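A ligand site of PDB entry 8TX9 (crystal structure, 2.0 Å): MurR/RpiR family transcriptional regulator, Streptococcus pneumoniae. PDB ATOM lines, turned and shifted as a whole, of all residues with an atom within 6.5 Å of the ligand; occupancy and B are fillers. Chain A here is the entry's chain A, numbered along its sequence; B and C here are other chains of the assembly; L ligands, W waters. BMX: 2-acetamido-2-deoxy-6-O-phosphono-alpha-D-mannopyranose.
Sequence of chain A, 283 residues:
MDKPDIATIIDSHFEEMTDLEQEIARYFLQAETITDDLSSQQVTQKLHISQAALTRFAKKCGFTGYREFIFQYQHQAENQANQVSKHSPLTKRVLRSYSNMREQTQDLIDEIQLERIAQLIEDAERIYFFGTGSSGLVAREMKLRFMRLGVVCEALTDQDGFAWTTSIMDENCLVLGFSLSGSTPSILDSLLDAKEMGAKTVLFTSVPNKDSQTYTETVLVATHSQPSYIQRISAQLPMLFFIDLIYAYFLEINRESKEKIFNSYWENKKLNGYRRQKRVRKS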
ATOM      1  N   GLY A 131     -20.159 -26.072  -6.579  1.00  0.00           N
ATOM      2  CA  GLY A 131     -20.974 -25.820  -7.781  1.00  0.00           C
ATOM      3  C   GLY A 131     -20.358 -26.545  -8.956  1.00  0.00           C
ATOM      4  O   GLY A 131     -19.187 -26.898  -8.937  1.00  0.00           O
ATOM      5  N   THR A 132     -21.177 -26.799  -9.966  1.00  0.00           N
ATOM      6  CA  THR A 132     -20.710 -27.455 -11.180  1.00  0.00           C
ATOM      7  C   THR A 132     -21.002 -26.557 -12.374  1.00  0.00           C
ATOM      8  O   THR A 132     -21.734 -25.580 -12.266  1.00  0.00           O
ATOM      9  CB  THR A 132     -21.352 -28.819 -11.391  1.00  0.00           C
ATOM     10  OG1 THR A 132     -22.754 -28.664 -11.626  1.00  0.00           O
ATOM     11  CG2 THR A 132     -21.131 -29.710 -10.136  1.00  0.00           C
ATOM     12  N   GLY A 133     -20.321 -26.844 -13.493  1.00  0.00           N
ATOM     13  CA  GLY A 133     -20.505 -26.039 -14.685  1.00  0.00           C
ATOM     14  C   GLY A 133     -20.330 -24.561 -14.361  1.00  0.00           C
ATOM     15  O   GLY A 133     -19.484 -24.189 -13.555  1.00  0.00           O
ATOM     16  N   SER A 134     -21.251 -23.715 -14.857  1.00  0.00           N
ATOM     17  CA  SER A 134     -21.140 -22.279 -14.611  1.00  0.00           C
ATOM     18  C   SER A 134     -21.242 -21.951 -13.129  1.00  0.00           C
ATOM     19  O   SER A 134     -20.607 -20.985 -12.663  1.00  0.00           O
ATOM     20  CB  SER A 134     -22.228 -21.523 -15.412  1.00  0.00           C
ATOM     21  OG  SER A 134     -21.886 -21.457 -16.793  1.00  0.00           O
ATOM     22  N   SER A 135     -22.034 -22.733 -12.387  1.00  0.00           N
ATOM     23  CA  SER A 135     -22.141 -22.576 -10.932  1.00  0.00           C
ATOM     24  C   SER A 135     -20.820 -22.843 -10.194  1.00  0.00           C
ATOM     25  O   SER A 135     -20.625 -22.366  -9.068  1.00  0.00           O
ATOM     26  CB  SER A 135     -23.245 -23.517 -10.386  1.00  0.00           C
ATOM     27  OG  SER A 135     -24.523 -23.129 -10.838  1.00  0.00           O
ATOM     28  N   GLY A 136     -19.970 -23.710 -10.747  1.00  0.00           N
ATOM     29  CA  GLY A 136     -18.599 -23.835 -10.240  1.00  0.00           C
ATOM     30  C   GLY A 136     -17.778 -22.554 -10.377  1.00  0.00           C
ATOM     31  O   GLY A 136     -16.945 -22.234  -9.516  1.00  0.00           O
ATOM     32  N   PHE A 178     -24.374 -24.162  -4.977  1.00  0.00           N
ATOM     33  CA  PHE A 178     -24.888 -23.365  -6.085  1.00  0.00           C
ATOM     34  C   PHE A 178     -25.446 -24.272  -7.165  1.00  0.00           C
ATOM     35  O   PHE A 178     -24.687 -24.974  -7.850  1.00  0.00           O
ATOM     36  CB  PHE A 178     -23.775 -22.484  -6.666  1.00  0.00           C
ATOM     37  CG  PHE A 178     -23.230 -21.442  -5.697  1.00  0.00           C
ATOM     38  CD1 PHE A 178     -23.860 -20.205  -5.557  1.00  0.00           C
ATOM     39  CD2 PHE A 178     -22.084 -21.629  -4.984  1.00  0.00           C
ATOM     40  CE1 PHE A 178     -23.360 -19.223  -4.730  1.00  0.00           C
ATOM     41  CE2 PHE A 178     -21.619 -20.657  -4.088  1.00  0.00           C
ATOM     42  CZ  PHE A 178     -22.271 -19.458  -3.973  1.00  0.00           C
ATOM     43  N   SER A 179     -26.758 -24.205  -7.382  1.00  0.00           N
ATOM     44  CA  SER A 179     -27.389 -24.999  -8.438  1.00  0.00           C
ATOM     45  C   SER A 179     -28.538 -24.146  -8.960  1.00  0.00           C
ATOM     46  O   SER A 179     -29.542 -23.944  -8.270  1.00  0.00           O
ATOM     47  CB  SER A 179     -27.854 -26.356  -7.911  1.00  0.00           C
ATOM     48  OG  SER A 179     -28.483 -27.175  -8.915  1.00  0.00           O
ATOM     49  N   LEU A 180     -28.314 -23.521 -10.113  1.00  0.00           N
ATOM     50  CA  LEU A 180     -29.327 -22.611 -10.628  1.00  0.00           C
ATOM     51  C   LEU A 180     -30.631 -23.364 -10.896  1.00  0.00           C
ATOM     52  O   LEU A 180     -31.694 -22.948 -10.430  1.00  0.00           O
ATOM     53  CB  LEU A 180     -28.819 -21.956 -11.893  1.00  0.00           C
ATOM     54  CG  LEU A 180     -29.520 -20.655 -12.239  1.00  0.00           C
ATOM     55  CD1 LEU A 180     -28.988 -19.559 -11.374  1.00  0.00           C
ATOM     56  CD2 LEU A 180     -29.258 -20.350 -13.695  1.00  0.00           C
ATOM     57  N   SER A 181     -30.537 -24.541 -11.545  1.00  0.00           N
ATOM     58  CA  SER A 181     -31.696 -25.386 -11.798  1.00  0.00           C
ATOM     59  C   SER A 181     -32.323 -25.989 -10.529  1.00  0.00           C
ATOM     60  O   SER A 181     -33.476 -26.422 -10.569  1.00  0.00           O
ATOM     61  CB  SER A 181     -31.346 -26.510 -12.790  1.00  0.00           C
ATOM     62  OG  SER A 181     -30.438 -27.470 -12.238  1.00  0.00           O
ATOM     63  N   GLY A 182     -31.553 -26.082  -9.426  1.00  0.00           N
ATOM     64  CA  GLY A 182     -31.966 -26.708  -8.176  1.00  0.00           C
ATOM     65  C   GLY A 182     -32.124 -28.214  -8.242  1.00  0.00           C
ATOM     66  O   GLY A 182     -32.575 -28.831  -7.259  1.00  0.00           O
ATOM     67  N   SER A 183     -31.692 -28.830  -9.317  1.00  0.00           N
ATOM     68  CA  SER A 183     -31.918 -30.248  -9.549  1.00  0.00           C
ATOM     69  C   SER A 183     -30.645 -31.078  -9.662  1.00  0.00           C
ATOM     70  O   SER A 183     -30.742 -32.311  -9.711  1.00  0.00           O
ATOM     71  CB  SER A 183     -32.707 -30.407 -10.853  1.00  0.00           C
ATOM     72  OG  SER A 183     -31.894 -30.069 -11.969  1.00  0.00           O
ATOM     73  N   THR A 184     -29.472 -30.439  -9.657  1.00  0.00           N
ATOM     74  CA  THR A 184     -28.224 -31.179  -9.840  1.00  0.00           C
ATOM     75  C   THR A 184     -27.966 -32.078  -8.635  1.00  0.00           C
ATOM     76  O   THR A 184     -27.808 -31.586  -7.516  1.00  0.00           O
ATOM     77  CB  THR A 184     -27.084 -30.197 -10.069  1.00  0.00           C
ATOM     78  OG1 THR A 184     -27.368 -29.428 -11.264  1.00  0.00           O
ATOM     79  CG2 THR A 184     -25.775 -30.951 -10.264  1.00  0.00           C
ATOM     80  N   ILE A 187     -24.955 -31.747  -6.014  1.00  0.00           N
ATOM     81  CA  ILE A 187     -24.974 -30.594  -5.114  1.00  0.00           C
ATOM     82  C   ILE A 187     -25.960 -30.815  -3.970  1.00  0.00           C
ATOM     83  O   ILE A 187     -25.653 -30.574  -2.802  1.00  0.00           O
ATOM     84  CB  ILE A 187     -25.348 -29.307  -5.887  1.00  0.00           C
ATOM     85  CG1 ILE A 187     -24.380 -28.994  -7.037  1.00  0.00           C
ATOM     86  CG2 ILE A 187     -25.463 -28.178  -4.864  1.00  0.00           C
ATOM     87  CD1 ILE A 187     -22.974 -28.472  -6.606  1.00  0.00           C
ATOM     88  N   TYR A 229     -32.962 -22.600 -24.023  1.00  0.00           N
ATOM     89  CA  TYR A 229     -31.810 -22.697 -23.146  1.00  0.00           C
ATOM     90  C   TYR A 229     -30.563 -22.117 -23.821  1.00  0.00           C
ATOM     91  O   TYR A 229     -29.789 -21.398 -23.185  1.00  0.00           O
ATOM     92  CB  TYR A 229     -31.500 -24.151 -22.724  1.00  0.00           C
ATOM     93  CG  TYR A 229     -31.148 -24.325 -21.256  1.00  0.00           C
ATOM     94  CD1 TYR A 229     -30.456 -23.304 -20.595  1.00  0.00           C
ATOM     95  CD2 TYR A 229     -31.705 -25.351 -20.460  1.00  0.00           C
ATOM     96  CE1 TYR A 229     -30.205 -23.353 -19.253  1.00  0.00           C
ATOM     97  CE2 TYR A 229     -31.436 -25.411 -19.097  1.00  0.00           C
ATOM     98  CZ  TYR A 229     -30.559 -24.479 -18.521  1.00  0.00           C
ATOM     99  OH  TYR A 229     -30.242 -24.535 -17.173  1.00  0.00           O
ATOM    100  N   ALA A 235     -25.035 -18.033 -17.215  1.00  0.00           N
ATOM    101  CA  ALA A 235     -25.683 -18.676 -16.069  1.00  0.00           C
ATOM    102  C   ALA A 235     -25.187 -18.184 -14.725  1.00  0.00           C
ATOM    103  O   ALA A 235     -25.914 -18.313 -13.719  1.00  0.00           O
ATOM    104  CB  ALA A 235     -25.472 -20.191 -16.191  1.00  0.00           C
ATOM    105  N   MET A 239     -26.544 -15.472  -9.673  1.00  0.00           N
ATOM    106  CA  MET A 239     -25.783 -15.719  -8.468  1.00  0.00           C
ATOM    107  C   MET A 239     -24.828 -14.574  -8.123  1.00  0.00           C
ATOM    108  O   MET A 239     -24.699 -14.201  -6.952  1.00  0.00           O
ATOM    109  CB  MET A 239     -24.963 -16.987  -8.595  1.00  0.00           C
ATOM    110  CG  MET A 239     -25.164 -18.031  -7.518  1.00  0.00           C
ATOM    111  SD  MET A 239     -26.578 -19.016  -7.969  1.00  0.00           S
ATOM    112  CE  MET A 239     -25.836 -19.914  -9.381  1.00  0.00           C
ATOM    113  N   LEU B 144     -16.734 -22.633 -22.058  1.00  0.00           N
ATOM    114  CA  LEU B 144     -17.864 -23.513 -21.835  1.00  0.00           C
ATOM    115  C   LEU B 144     -18.944 -23.264 -22.874  1.00  0.00           C
ATOM    116  O   LEU B 144     -19.411 -24.191 -23.533  1.00  0.00           O
ATOM    117  CB  LEU B 144     -18.398 -23.314 -20.418  1.00  0.00           C
ATOM    118  CG  LEU B 144     -19.456 -24.257 -19.852  1.00  0.00           C
ATOM    119  CD1 LEU B 144     -19.344 -24.190 -18.326  1.00  0.00           C
ATOM    120  CD2 LEU B 144     -20.904 -23.947 -20.316  1.00  0.00           C
ATOM    121  N   ARG B 148     -19.918 -25.557 -26.680  1.00  0.00           N
ATOM    122  CA  ARG B 148     -21.263 -26.112 -26.842  1.00  0.00           C
ATOM    123  C   ARG B 148     -21.945 -25.669 -28.139  1.00  0.00           C
ATOM    124  O   ARG B 148     -23.025 -26.180 -28.457  1.00  0.00           O
ATOM    125  CB  ARG B 148     -22.148 -25.724 -25.659  1.00  0.00           C
ATOM    126  CG  ARG B 148     -21.606 -26.273 -24.373  1.00  0.00           C
ATOM    127  CD  ARG B 148     -22.443 -25.859 -23.211  1.00  0.00           C
ATOM    128  NE  ARG B 148     -23.668 -26.663 -23.132  1.00  0.00           N
ATOM    129  CZ  ARG B 148     -24.509 -26.605 -22.117  1.00  0.00           C
ATOM    130  NH1 ARG B 148     -24.312 -25.758 -21.112  1.00  0.00           N
ATOM    131  NH2 ARG B 148     -25.547 -27.440 -22.078  1.00  0.00           N
ATOM    132  N   PHE B 262     -25.452 -27.985 -29.529  1.00  0.00           N
ATOM    133  CA  PHE B 262     -25.890 -27.620 -28.198  1.00  0.00           C
ATOM    134  C   PHE B 262     -26.769 -28.701 -27.599  1.00  0.00           C
ATOM    135  O   PHE B 262     -26.593 -29.104 -26.450  1.00  0.00           O
ATOM    136  CB  PHE B 262     -26.650 -26.327 -28.228  1.00  0.00           C
ATOM    137  CG  PHE B 262     -26.949 -25.779 -26.880  1.00  0.00           C
ATOM    138  CD1 PHE B 262     -25.966 -25.131 -26.145  1.00  0.00           C
ATOM    139  CD2 PHE B 262     -28.227 -25.834 -26.373  1.00  0.00           C
ATOM    140  CE1 PHE B 262     -26.254 -24.589 -24.897  1.00  0.00           C
ATOM    141  CE2 PHE B 262     -28.530 -25.278 -25.136  1.00  0.00           C
ATOM    142  CZ  PHE B 262     -27.550 -24.680 -24.382  1.00  0.00           C
ATOM    143  N   TYR B 265     -26.337 -32.601 -25.777  1.00  0.00           N
ATOM    144  CA  TYR B 265     -26.074 -32.764 -24.332  1.00  0.00           C
ATOM    145  C   TYR B 265     -27.305 -33.318 -23.637  1.00  0.00           C
ATOM    146  O   TYR B 265     -27.195 -34.295 -22.891  1.00  0.00           O
ATOM    147  CB  TYR B 265     -25.665 -31.422 -23.718  1.00  0.00           C
ATOM    148  CG  TYR B 265     -25.469 -31.489 -22.223  1.00  0.00           C
ATOM    149  CD1 TYR B 265     -24.517 -32.330 -21.660  1.00  0.00           C
ATOM    150  CD2 TYR B 265     -26.239 -30.707 -21.365  1.00  0.00           C
ATOM    151  CE1 TYR B 265     -24.331 -32.395 -20.295  1.00  0.00           C
ATOM    152  CE2 TYR B 265     -26.059 -30.764 -19.990  1.00  0.00           C
ATOM    153  CZ  TYR B 265     -25.102 -31.612 -19.459  1.00  0.00           C
ATOM    154  OH  TYR B 265     -24.919 -31.700 -18.118  1.00  0.00           O
ATOM    155  N   TRP B 266     -28.462 -32.685 -23.870  1.00  0.00           N
ATOM    156  CA  TRP B 266     -29.718 -33.109 -23.237  1.00  0.00           C
ATOM    157  C   TRP B 266     -30.185 -34.414 -23.837  1.00  0.00           C
ATOM    158  O   TRP B 266     -30.841 -35.194 -23.123  1.00  0.00           O
ATOM    159  CB  TRP B 266     -30.794 -32.045 -23.460  1.00  0.00           C
ATOM    160  CG  TRP B 266     -30.678 -30.854 -22.567  1.00  0.00           C
ATOM    161  CD1 TRP B 266     -31.335 -30.635 -21.386  1.00  0.00           C
ATOM    162  CD2 TRP B 266     -29.860 -29.690 -22.794  1.00  0.00           C
ATOM    163  NE1 TRP B 266     -30.982 -29.422 -20.864  1.00  0.00           N
ATOM    164  CE2 TRP B 266     -30.073 -28.829 -21.692  1.00  0.00           C
ATOM    165  CE3 TRP B 266     -28.969 -29.311 -23.793  1.00  0.00           C
ATOM    166  CZ2 TRP B 266     -29.435 -27.601 -21.584  1.00  0.00           C
ATOM    167  CZ3 TRP B 266     -28.335 -28.091 -23.681  1.00  0.00           C
ATOM    168  CH2 TRP B 266     -28.581 -27.246 -22.597  1.00  0.00           C
ATOM    169  N   ASP C 160     -19.279 -33.398 -17.283  1.00  0.00           N
ATOM    170  CA  ASP C 160     -19.779 -32.411 -18.243  1.00  0.00           C
ATOM    171  C   ASP C 160     -18.747 -32.156 -19.346  1.00  0.00           C
ATOM    172  O   ASP C 160     -19.027 -32.304 -20.544  1.00  0.00           O
ATOM    173  CB  ASP C 160     -20.130 -31.130 -17.505  1.00  0.00           C
ATOM    174  CG  ASP C 160     -21.485 -31.215 -16.767  1.00  0.00           C
ATOM    175  OD1 ASP C 160     -22.319 -32.078 -17.138  1.00  0.00           O
ATOM    176  OD2 ASP C 160     -21.752 -30.359 -15.879  1.00  0.00           O
ATOM    177  N   TRP C 164     -19.423 -32.607 -23.695  1.00  0.00           N
ATOM    178  CA  TRP C 164     -19.297 -31.471 -24.620  1.00  0.00           C
ATOM    179  C   TRP C 164     -18.135 -31.663 -25.567  1.00  0.00           C
ATOM    180  O   TRP C 164     -18.159 -31.218 -26.696  1.00  0.00           O
ATOM    181  CB  TRP C 164     -19.095 -30.176 -23.821  1.00  0.00           C
ATOM    182  CG  TRP C 164     -20.230 -29.923 -22.969  1.00  0.00           C
ATOM    183  CD1 TRP C 164     -21.531 -30.262 -23.221  1.00  0.00           C
ATOM    184  CD2 TRP C 164     -20.250 -29.187 -21.745  1.00  0.00           C
ATOM    185  NE1 TRP C 164     -22.337 -29.881 -22.166  1.00  0.00           N
ATOM    186  CE2 TRP C 164     -21.593 -29.126 -21.293  1.00  0.00           C
ATOM    187  CE3 TRP C 164     -19.253 -28.537 -20.992  1.00  0.00           C
ATOM    188  CZ2 TRP C 164     -21.966 -28.480 -20.124  1.00  0.00           C
ATOM    189  CZ3 TRP C 164     -19.634 -27.910 -19.793  1.00  0.00           C
ATOM    190  CH2 TRP C 164     -20.976 -27.883 -19.384  1.00  0.00           C
HETATM  191  C1  BMX L   1     -24.874 -27.990 -16.777  1.00  0.00           C
HETATM  192  C2  BMX L   1     -24.727 -26.812 -17.744  1.00  0.00           C
HETATM  193  C3  BMX L   1     -24.400 -25.497 -17.097  1.00  0.00           C
HETATM  194  C4  BMX L   1     -24.842 -25.422 -15.661  1.00  0.00           C
HETATM  195  C5  BMX L   1     -24.363 -26.653 -14.839  1.00  0.00           C
HETATM  196  C6  BMX L   1     -25.494 -27.219 -14.091  1.00  0.00           C
HETATM  197  C7  BMX L   1     -27.322 -26.547 -18.158  1.00  0.00           C
HETATM  198  C8  BMX L   1     -27.814 -26.399 -16.701  1.00  0.00           C
HETATM  199  N2  BMX L   1     -25.952 -26.741 -18.624  1.00  0.00           N
HETATM  200  O1  BMX L   1     -24.540 -29.154 -17.398  1.00  0.00           O
HETATM  201  O3  BMX L   1     -24.997 -24.383 -17.855  1.00  0.00           O
HETATM  202  O4  BMX L   1     -24.428 -24.197 -15.028  1.00  0.00           O
HETATM  203  O5  BMX L   1     -23.938 -27.793 -15.637  1.00  0.00           O
HETATM  204  O6  BMX L   1     -25.504 -26.655 -12.829  1.00  0.00           O
HETATM  205  O7  BMX L   1     -28.114 -26.505 -19.017  1.00  0.00           O
HETATM  206  P   BMX L   1     -26.907 -25.985 -12.359  1.00  0.00           P
HETATM  207  O19 BMX L   1     -28.087 -26.364 -13.278  1.00  0.00           O
HETATM  208  O17 BMX L   1     -27.221 -26.438 -10.957  1.00  0.00           O
HETATM  209  O18 BMX L   1     -26.732 -24.496 -12.259  1.00  0.00           O
HETATM  210  O   HOH W   1     -23.990 -27.027  -9.792  1.00  0.00           O
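The side-chain carboxylate of Asp 160 of chain C sits at hydrogen-bond distance from the side-chain hydroxyl of Tyr 265 of chain B. OG of Ser 179 is in hydrogen-bond range of N of Gly 182 (3.3 Å). The side-chain hydroxyl of Ser 183 lies within hydrogen-bond range of the side-chain hydroxyl of Ser 181 (3.0 Å). The side-chain hydroxyl of Thr 184 lies within hydrogen-bond range of the side-chain hydroxyl of Ser 179. The backbone NH of Phe 262 of chain B lies within hydrogen-bond range of the backbone carbonyl oxygen of Arg 148 of chain B (3.2 Å).
The guanidinium group of Arg 148 of chain B lies close to a nitrogen (N2) of the ligand. Merely in contact with the ligand: Trp 266 of chain B (3.1 Å), Thr 132 (3.6 Å), Trp 164 of chain C (3.8 Å) and Gly 133 (3.9 Å). Hydrophobic or aromatic side chains within 4 Å of the ligand: Leu 180, Tyr 229, Tyr 265 of chain B, Trp 266 of chain B and Trp 164 of chain C. Within 4 Å of the ligand: Thr 132, Gly 133, Ser 134, Ser 135, Ser 179, Leu 180, Ser 181, Thr 184, Tyr 229, Arg 148 of chain B, Tyr 265 of chain B, Trp 266 of chain B, Asp 160 of chain C and Trp 164 of chain C.
Water W1 lies within hydrogen-bond range of the side-chain hydroxyl (OG1) of Thr 132 (2.8 Å), the backbone carbonyl oxygen (O) of Phe 178 (2.9 Å) and an oxygen (O6) of the ligand (3.4 Å).
The backbone NH (N) of Leu 180 sits at hydrogen-bond distance from an oxygen (O18) of the ligand (2.8 Å). OH of Tyr 265 of chain B sits at hydrogen-bond distance from O1 of the ligand (2.7 Å). OH of Tyr 229 sits close to O7 of the ligand (3.4 Å). The side-chain hydroxyl (OG1) of Thr 184 is in hydrogen-bond range of an oxygen (O17) of the ligand, 3.0 Å away. The backbone NH (N) of Ser 134 sits at hydrogen-bond distance from an oxygen (O4) of the ligand (3.2 Å). The side-chain hydroxyl (OG) of Ser 181 sits at hydrogen-bond distance from an oxygen (O19) of the ligand, 2.8 Å away. OG of Ser 135 lies within hydrogen-bond range of O18 of the ligand (3.0 Å). An oxygen (O17) of the ligand lies within hydrogen-bond range of the side-chain hydroxyl (OG) of Ser 179, at 2.5 Å. O1 of the ligand lies within hydrogen-bond range of OD2 of Asp 160 of chain C.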
